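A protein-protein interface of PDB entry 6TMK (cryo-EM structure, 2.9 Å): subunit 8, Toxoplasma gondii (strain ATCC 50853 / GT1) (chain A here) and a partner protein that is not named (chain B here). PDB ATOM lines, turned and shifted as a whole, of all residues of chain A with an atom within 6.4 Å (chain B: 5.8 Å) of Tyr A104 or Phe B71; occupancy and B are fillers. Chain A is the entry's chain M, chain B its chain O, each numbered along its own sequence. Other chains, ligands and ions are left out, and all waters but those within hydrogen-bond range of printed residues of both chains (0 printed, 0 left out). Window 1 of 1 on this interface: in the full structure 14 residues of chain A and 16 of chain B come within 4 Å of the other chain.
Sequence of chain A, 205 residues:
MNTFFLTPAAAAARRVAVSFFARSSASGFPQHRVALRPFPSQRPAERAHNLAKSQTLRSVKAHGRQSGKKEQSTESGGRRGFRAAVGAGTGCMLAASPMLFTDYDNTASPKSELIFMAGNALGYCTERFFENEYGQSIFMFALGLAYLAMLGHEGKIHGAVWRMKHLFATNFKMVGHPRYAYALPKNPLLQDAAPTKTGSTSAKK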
ATOM      1  N   PRO A  98      29.579  19.747   0.932  1.00  0.00           N
ATOM      2  CA  PRO A  98      28.463  19.618  -0.009  1.00  0.00           C
ATOM      3  C   PRO A  98      27.098  19.677   0.651  1.00  0.00           C
ATOM      4  O   PRO A  98      26.102  19.864  -0.056  1.00  0.00           O
ATOM      5  CB  PRO A  98      28.714  18.255  -0.667  1.00  0.00           C
ATOM      6  CG  PRO A  98      29.636  17.546   0.220  1.00  0.00           C
ATOM      7  CD  PRO A  98      30.442  18.561   0.932  1.00  0.00           C
ATOM      8  N   MET A  99      27.008  19.519   1.969  1.00  0.00           N
ATOM      9  CA  MET A  99      25.720  19.509   2.646  1.00  0.00           C
ATOM     10  C   MET A  99      25.227  20.892   3.050  1.00  0.00           C
ATOM     11  O   MET A  99      24.051  21.028   3.401  1.00  0.00           O
ATOM     12  CB  MET A  99      25.778  18.595   3.866  1.00  0.00           C
ATOM     13  CG  MET A  99      25.386  17.158   3.559  1.00  0.00           C
ATOM     14  SD  MET A  99      26.374  16.319   2.316  1.00  0.00           S
ATOM     15  CE  MET A  99      27.865  16.033   3.231  1.00  0.00           C
ATOM     16  N   PHE A 101      24.908  23.028   0.848  1.00  0.00           N
ATOM     17  CA  PHE A 101      24.079  23.272  -0.321  1.00  0.00           C
ATOM     18  C   PHE A 101      22.702  22.657  -0.127  1.00  0.00           C
ATOM     19  O   PHE A 101      22.578  21.505   0.296  1.00  0.00           O
ATOM     20  CB  PHE A 101      24.752  22.705  -1.566  1.00  0.00           C
ATOM     21  CG  PHE A 101      24.121  23.147  -2.841  1.00  0.00           C
ATOM     22  CD1 PHE A 101      24.487  24.339  -3.424  1.00  0.00           C
ATOM     23  CD2 PHE A 101      23.170  22.371  -3.462  1.00  0.00           C
ATOM     24  CE1 PHE A 101      23.914  24.749  -4.589  1.00  0.00           C
ATOM     25  CE2 PHE A 101      22.594  22.779  -4.631  1.00  0.00           C
ATOM     26  CZ  PHE A 101      22.968  23.968  -5.198  1.00  0.00           C
ATOM     27  N   THR A 102      21.667  23.432  -0.445  1.00  0.00           N
ATOM     28  CA  THR A 102      20.293  22.981  -0.282  1.00  0.00           C
ATOM     29  C   THR A 102      19.489  23.146  -1.567  1.00  0.00           C
ATOM     30  O   THR A 102      18.558  22.375  -1.819  1.00  0.00           O
ATOM     31  CB  THR A 102      19.628  23.752   0.862  1.00  0.00           C
ATOM     32  OG1 THR A 102      18.282  23.296   1.034  1.00  0.00           O
ATOM     33  CG2 THR A 102      19.615  25.243   0.567  1.00  0.00           C
ATOM     34  N   ASP A 103      19.839  24.137  -2.388  1.00  0.00           N
ATOM     35  CA  ASP A 103      19.025  24.504  -3.548  1.00  0.00           C
ATOM     36  C   ASP A 103      19.254  23.499  -4.678  1.00  0.00           C
ATOM     37  O   ASP A 103      19.874  23.779  -5.706  1.00  0.00           O
ATOM     38  CB  ASP A 103      19.344  25.926  -3.991  1.00  0.00           C
ATOM     39  CG  ASP A 103      18.112  26.695  -4.447  1.00  0.00           C
ATOM     40  OD1 ASP A 103      17.017  26.099  -4.515  1.00  0.00           O
ATOM     41  OD2 ASP A 103      18.240  27.901  -4.743  1.00  0.00           O
ATOM     42  N   TYR A 104      18.711  22.301  -4.474  1.00  0.00           N
ATOM     43  CA  TYR A 104      18.877  21.198  -5.408  1.00  0.00           C
ATOM     44  C   TYR A 104      17.741  21.090  -6.413  1.00  0.00           C
ATOM     45  O   TYR A 104      17.896  20.406  -7.431  1.00  0.00           O
ATOM     46  CB  TYR A 104      18.992  19.869  -4.663  1.00  0.00           C
ATOM     47  CG  TYR A 104      20.402  19.442  -4.343  1.00  0.00           C
ATOM     48  CD1 TYR A 104      21.320  19.205  -5.352  1.00  0.00           C
ATOM     49  CD2 TYR A 104      20.807  19.248  -3.037  1.00  0.00           C
ATOM     50  CE1 TYR A 104      22.603  18.810  -5.068  1.00  0.00           C
ATOM     51  CE2 TYR A 104      22.086  18.850  -2.741  1.00  0.00           C
ATOM     52  CZ  TYR A 104      22.982  18.627  -3.758  1.00  0.00           C
ATOM     53  OH  TYR A 104      24.263  18.228  -3.458  1.00  0.00           O
ATOM     54  N   ASP A 105      16.607  21.732  -6.150  1.00  0.00           N
ATOM     55  CA  ASP A 105      15.407  21.569  -6.955  1.00  0.00           C
ATOM     56  C   ASP A 105      15.283  22.613  -8.054  1.00  0.00           C
ATOM     57  O   ASP A 105      14.224  22.710  -8.682  1.00  0.00           O
ATOM     58  CB  ASP A 105      14.170  21.611  -6.060  1.00  0.00           C
ATOM     59  CG  ASP A 105      14.196  20.550  -4.979  1.00  0.00           C
ATOM     60  OD1 ASP A 105      14.001  19.362  -5.311  1.00  0.00           O
ATOM     61  OD2 ASP A 105      14.410  20.899  -3.799  1.00  0.00           O
ATOM     62  N   ASN A 106      16.330  23.393  -8.298  1.00  0.00           N
ATOM     63  CA  ASN A 106      16.353  24.326  -9.422  1.00  0.00           C
ATOM     64  C   ASN A 106      16.965  23.643 -10.647  1.00  0.00           C
ATOM     65  O   ASN A 106      17.961  24.080 -11.219  1.00  0.00           O
ATOM     66  CB  ASN A 106      17.124  25.583  -9.045  1.00  0.00           C
ATOM     67  CG  ASN A 106      16.500  26.322  -7.888  1.00  0.00           C
ATOM     68  OD1 ASN A 106      15.444  25.937  -7.387  1.00  0.00           O
ATOM     69  ND2 ASN A 106      17.154  27.392  -7.448  1.00  0.00           N
ATOM     70  N   THR A 107      16.330  22.541 -11.044  1.00  0.00           N
ATOM     71  CA  THR A 107      16.822  21.689 -12.126  1.00  0.00           C
ATOM     72  C   THR A 107      16.260  22.186 -13.450  1.00  0.00           C
ATOM     73  O   THR A 107      15.231  21.716 -13.935  1.00  0.00           O
ATOM     74  CB  THR A 107      16.455  20.231 -11.884  1.00  0.00           C
ATOM     75  OG1 THR A 107      15.030  20.078 -11.916  1.00  0.00           O
ATOM     76  CG2 THR A 107      16.992  19.757 -10.562  1.00  0.00           C
ATOM     77  N   HIS B  69      22.273  16.761 -13.925  1.00  0.00           N
ATOM     78  CA  HIS B  69      22.077  18.132 -13.480  1.00  0.00           C
ATOM     79  C   HIS B  69      23.244  18.527 -12.588  1.00  0.00           C
ATOM     80  O   HIS B  69      23.463  17.914 -11.541  1.00  0.00           O
ATOM     81  CB  HIS B  69      20.752  18.304 -12.746  1.00  0.00           C
ATOM     82  CG  HIS B  69      19.554  18.064 -13.601  1.00  0.00           C
ATOM     83  ND1 HIS B  69      19.035  19.029 -14.434  1.00  0.00           N
ATOM     84  CD2 HIS B  69      18.751  16.982 -13.729  1.00  0.00           C
ATOM     85  CE1 HIS B  69      17.977  18.543 -15.058  1.00  0.00           C
ATOM     86  NE2 HIS B  69      17.783  17.305 -14.647  1.00  0.00           N
ATOM     87  N   VAL B  70      23.986  19.545 -13.001  1.00  0.00           N
ATOM     88  CA  VAL B  70      25.237  19.925 -12.363  1.00  0.00           C
ATOM     89  C   VAL B  70      25.013  21.189 -11.549  1.00  0.00           C
ATOM     90  O   VAL B  70      24.340  22.125 -11.995  1.00  0.00           O
ATOM     91  CB  VAL B  70      26.356  20.123 -13.399  1.00  0.00           C
ATOM     92  CG1 VAL B  70      27.609  20.621 -12.734  1.00  0.00           C
ATOM     93  CG2 VAL B  70      26.626  18.836 -14.122  1.00  0.00           C
ATOM     94  N   PHE B  71      25.584  21.206 -10.349  1.00  0.00           N
ATOM     95  CA  PHE B  71      25.523  22.330  -9.435  1.00  0.00           C
ATOM     96  C   PHE B  71      26.926  22.630  -8.937  1.00  0.00           C
ATOM     97  O   PHE B  71      27.813  21.779  -8.981  1.00  0.00           O
ATOM     98  CB  PHE B  71      24.624  22.039  -8.236  1.00  0.00           C
ATOM     99  CG  PHE B  71      23.231  21.648  -8.596  1.00  0.00           C
ATOM    100  CD1 PHE B  71      22.199  22.552  -8.503  1.00  0.00           C
ATOM    101  CD2 PHE B  71      22.950  20.367  -9.011  1.00  0.00           C
ATOM    102  CE1 PHE B  71      20.925  22.189  -8.827  1.00  0.00           C
ATOM    103  CE2 PHE B  71      21.677  20.004  -9.336  1.00  0.00           C
ATOM    104  CZ  PHE B  71      20.663  20.916  -9.245  1.00  0.00           C
ATOM    105  N   ILE B  72      27.122  23.851  -8.455  1.00  0.00           N
ATOM    106  CA  ILE B  72      28.386  24.259  -7.863  1.00  0.00           C
ATOM    107  C   ILE B  72      28.115  24.899  -6.511  1.00  0.00           C
ATOM    108  O   ILE B  72      27.137  25.636  -6.343  1.00  0.00           O
ATOM    109  CB  ILE B  72      29.158  25.216  -8.789  1.00  0.00           C
ATOM    110  CG1 ILE B  72      29.640  24.459 -10.019  1.00  0.00           C
ATOM    111  CG2 ILE B  72      30.332  25.811  -8.072  1.00  0.00           C
ATOM    112  CD1 ILE B  72      30.041  25.322 -11.151  1.00  0.00           C
ATOM    113  N   ASN B  73      28.991  24.614  -5.546  1.00  0.00           N
ATOM    114  CA  ASN B  73      28.766  25.032  -4.168  1.00  0.00           C
ATOM    115  C   ASN B  73      28.859  26.544  -4.019  1.00  0.00           C
ATOM    116  O   ASN B  73      27.997  27.170  -3.392  1.00  0.00           O
ATOM    117  CB  ASN B  73      29.785  24.342  -3.261  1.00  0.00           C
ATOM    118  CG  ASN B  73      29.351  24.286  -1.820  1.00  0.00           C
ATOM    119  OD1 ASN B  73      29.899  24.983  -0.970  1.00  0.00           O
ATOM    120  ND2 ASN B  73      28.375  23.443  -1.529  1.00  0.00           N
ATOM    121  N   TRP B  90      27.223  31.361 -15.572  1.00  0.00           N
ATOM    122  CA  TRP B  90      26.859  30.031 -15.119  1.00  0.00           C
ATOM    123  C   TRP B  90      25.549  30.067 -14.347  1.00  0.00           C
ATOM    124  O   TRP B  90      25.284  30.999 -13.584  1.00  0.00           O
ATOM    125  CB  TRP B  90      27.959  29.453 -14.232  1.00  0.00           C
ATOM    126  CG  TRP B  90      27.586  28.157 -13.603  1.00  0.00           C
ATOM    127  CD1 TRP B  90      27.059  27.976 -12.365  1.00  0.00           C
ATOM    128  CD2 TRP B  90      27.710  26.857 -14.180  1.00  0.00           C
ATOM    129  NE1 TRP B  90      26.842  26.644 -12.133  1.00  0.00           N
ATOM    130  CE2 TRP B  90      27.235  25.936 -13.235  1.00  0.00           C
ATOM    131  CE3 TRP B  90      28.174  26.384 -15.404  1.00  0.00           C
ATOM    132  CZ2 TRP B  90      27.211  24.574 -13.475  1.00  0.00           C
ATOM    133  CZ3 TRP B  90      28.150  25.032 -15.637  1.00  0.00           C
ATOM    134  CH2 TRP B  90      27.674  24.144 -14.681  1.00  0.00           C
ATOM    135  N   ASN B  92      23.079  27.223 -12.051  1.00  0.00           N
ATOM    136  CA  ASN B  92      23.052  25.900 -11.454  1.00  0.00           C
ATOM    137  C   ASN B  92      21.810  25.140 -11.890  1.00  0.00           C
ATOM    138  O   ASN B  92      20.743  25.719 -12.110  1.00  0.00           O
ATOM    139  CB  ASN B  92      23.096  25.990  -9.932  1.00  0.00           C
ATOM    140  CG  ASN B  92      24.488  26.187  -9.403  1.00  0.00           C
ATOM    141  OD1 ASN B  92      25.473  25.975 -10.105  1.00  0.00           O
ATOM    142  ND2 ASN B  92      24.581  26.592  -8.151  1.00  0.00           N
ATOM    143  N   GLY B  93      21.958  23.827 -12.006  1.00  0.00           N
ATOM    144  CA  GLY B  93      20.902  22.978 -12.501  1.00  0.00           C
ATOM    145  C   GLY B  93      20.984  22.677 -13.971  1.00  0.00           C
ATOM    146  O   GLY B  93      20.040  22.103 -14.522  1.00  0.00           O
ATOM    147  N   ALA B 124      30.433  15.379  -6.042  1.00  0.00           N
ATOM    148  CA  ALA B 124      29.659  14.624  -5.076  1.00  0.00           C
ATOM    149  C   ALA B 124      28.252  14.408  -5.601  1.00  0.00           C
ATOM    150  O   ALA B 124      27.760  15.141  -6.458  1.00  0.00           O
ATOM    151  CB  ALA B 124      29.595  15.330  -3.723  1.00  0.00           C
ATOM    152  N   ARG B 126      24.651  13.148  -3.599  1.00  0.00           N
ATOM    153  CA  ARG B 126      23.969  12.678  -2.403  1.00  0.00           C
ATOM    154  C   ARG B 126      24.938  12.546  -1.236  1.00  0.00           C
ATOM    155  O   ARG B 126      24.793  11.666  -0.386  1.00  0.00           O
ATOM    156  CB  ARG B 126      23.258  11.354  -2.678  1.00  0.00           C
ATOM    157  CG  ARG B 126      22.210  10.975  -1.682  1.00  0.00           C
ATOM    158  CD  ARG B 126      21.134  10.148  -2.337  1.00  0.00           C
ATOM    159  NE  ARG B 126      20.127  11.001  -2.949  1.00  0.00           N
ATOM    160  CZ  ARG B 126      19.018  11.403  -2.338  1.00  0.00           C
ATOM    161  NH1 ARG B 126      18.764  11.033  -1.092  1.00  0.00           N
ATOM    162  NH2 ARG B 126      18.161  12.186  -2.970  1.00  0.00           N
ATOM    163  N   GLY B 127      25.924  13.435  -1.185  1.00  0.00           N
ATOM    164  CA  GLY B 127      26.862  13.496  -0.094  1.00  0.00           C
ATOM    165  C   GLY B 127      28.089  12.629  -0.235  1.00  0.00           C
ATOM    166  O   GLY B 127      28.874  12.539   0.716  1.00  0.00           O
ATOM    167  N   ARG B 149      21.933  14.195  -9.733  1.00  0.00           N
ATOM    168  CA  ARG B 149      22.306  15.562  -9.404  1.00  0.00           C
ATOM    169  C   ARG B 149      23.715  15.621  -8.827  1.00  0.00           C
ATOM    170  O   ARG B 149      23.942  15.216  -7.684  1.00  0.00           O
ATOM    171  CB  ARG B 149      21.287  16.148  -8.435  1.00  0.00           C
ATOM    172  CG  ARG B 149      19.899  16.232  -9.015  1.00  0.00           C
ATOM    173  CD  ARG B 149      18.891  16.687  -8.001  1.00  0.00           C
ATOM    174  NE  ARG B 149      18.728  15.703  -6.940  1.00  0.00           N
ATOM    175  CZ  ARG B 149      17.658  15.610  -6.160  1.00  0.00           C
ATOM    176  NH1 ARG B 149      16.644  16.445  -6.311  1.00  0.00           N
ATOM    177  NH2 ARG B 149      17.606  14.676  -5.225  1.00  0.00           N
ATOM    178  N   LEU B 150      24.659  16.135  -9.606  1.00  0.00           N
ATOM    179  CA  LEU B 150      26.048  16.260  -9.195  1.00  0.00           C
ATOM    180  C   LEU B 150      26.332  17.646  -8.635  1.00  0.00           C
ATOM    181  O   LEU B 150      25.727  18.638  -9.045  1.00  0.00           O
ATOM    182  CB  LEU B 150      26.989  15.976 -10.363  1.00  0.00           C
ATOM    183  CG  LEU B 150      26.700  14.707 -11.155  1.00  0.00           C
ATOM    184  CD1 LEU B 150      27.722  14.505 -12.236  1.00  0.00           C
ATOM    185  CD2 LEU B 150      26.668  13.512 -10.238  1.00  0.00           C
ATOM    186  N   LEU B 151      27.278  17.704  -7.705  1.00  0.00           N
ATOM    187  CA  LEU B 151      27.692  18.947  -7.081  1.00  0.00           C
ATOM    188  C   LEU B 151      29.207  19.058  -7.104  1.00  0.00           C
ATOM    189  O   LEU B 151      29.911  18.095  -6.797  1.00  0.00           O
ATOM    190  CB  LEU B 151      27.208  19.019  -5.640  1.00  0.00           C
ATOM    191  CG  LEU B 151      27.537  20.287  -4.869  1.00  0.00           C
ATOM    192  CD1 LEU B 151      26.607  21.403  -5.248  1.00  0.00           C
ATOM    193  CD2 LEU B 151      27.469  20.008  -3.410  1.00  0.00           C
ATOM    194  N   LEU B 152      29.702  20.234  -7.464  1.00  0.00           N
ATOM    195  CA  LEU B 152      31.128  20.523  -7.475  1.00  0.00           C
ATOM    196  C   LEU B 152      31.467  21.396  -6.278  1.00  0.00           C
ATOM    197  O   LEU B 152      30.892  22.477  -6.110  1.00  0.00           O
ATOM    198  CB  LEU B 152      31.527  21.218  -8.772  1.00  0.00           C
ATOM    199  CG  LEU B 152      31.902  20.311  -9.929  1.00  0.00           C
ATOM    200  CD1 LEU B 152      30.699  19.534 -10.368  1.00  0.00           C
ATOM    201  CD2 LEU B 152      32.415  21.154 -11.050  1.00  0.00           C
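A ring nitrogen (ND1) of His B69 lies within hydrogen-bond range of the backbone carbonyl oxygen of Gly B93. The backbone carbonyl oxygen (O) of Val B70 lies within hydrogen-bond range of the backbone NH (N) of Gly B93 (2.9 Å). The backbone carbonyl oxygen (O) of Leu B150 sits at hydrogen-bond distance from the backbone NH (N) of Phe B71. The side-chain amide oxygen (OD1) of Asn B92 sits at hydrogen-bond distance from the backbone NH (N) of Ile B72 (3.2 Å). The side-chain amide oxygen (OD1) of Asn B92 lies within hydrogen-bond range of the indole nitrogen (NE1) of Trp B90 (2.5 Å). O of Leu B151 lies within hydrogen-bond range of N of Ala B124, at 2.9 Å.
O of Asn A106 lies close to O of Asn B92 (3.3 Å).
Among the printed residues, merely in contact across the chains: Pro A98 with Leu B151 (3.5 Å), Met A99 with Gly B127 (3.7 Å), Phe A101 with Phe B71 (3.7 Å), Phe A101 with Ile B72 (3.8 Å), Phe A101 with Asn B73 (3.7 Å), Phe A101 with Leu B151 (3.9 Å), Asp A103 with Phe B71 (3.7 Å), Tyr A104 with Phe B71 (3.3 Å), Tyr A104 with Arg B149 (3.9 Å), Tyr A104 with Leu B151 (3.7 Å), Asn A106 with Gly B93 (3.4 Å), Thr A107 with His B69 (3.8 Å) and Thr A107 with Gly B93 (3.9 Å).
Printed residues of chain B within 4 Å of Asp A103: Phe B71 (3.7 Å). Tyr A104 touches three residues of chain B. Phe B71 touches just these residues of chain A: Phe A101, Asp A103 and Tyr A104. Printed residues of chain A within 4 Å of Ile B72: Phe A101 (3.8 Å). Of the printed residues of chain A, Gly B93 touches Asn A106 and Thr A107. Arg B126 touches none of the printed residues of chain A. Of the printed residues of chain A, Arg B149 touches Tyr A104. Leu B152 touches none of the printed residues of chain A. The nearest printed residue of chain A that does not touch His B69 is Asn A106 (6.1 Å).
Of the 9 printed residues of chain A, 7 touch a printed residue of chain B. Hydrophobic or aromatic side chains of chain A that line the printed part of chain B: Pro A98, Met A99, Phe A101 and Tyr A104. Among the printed residues, 14 pairs touch across the chains.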
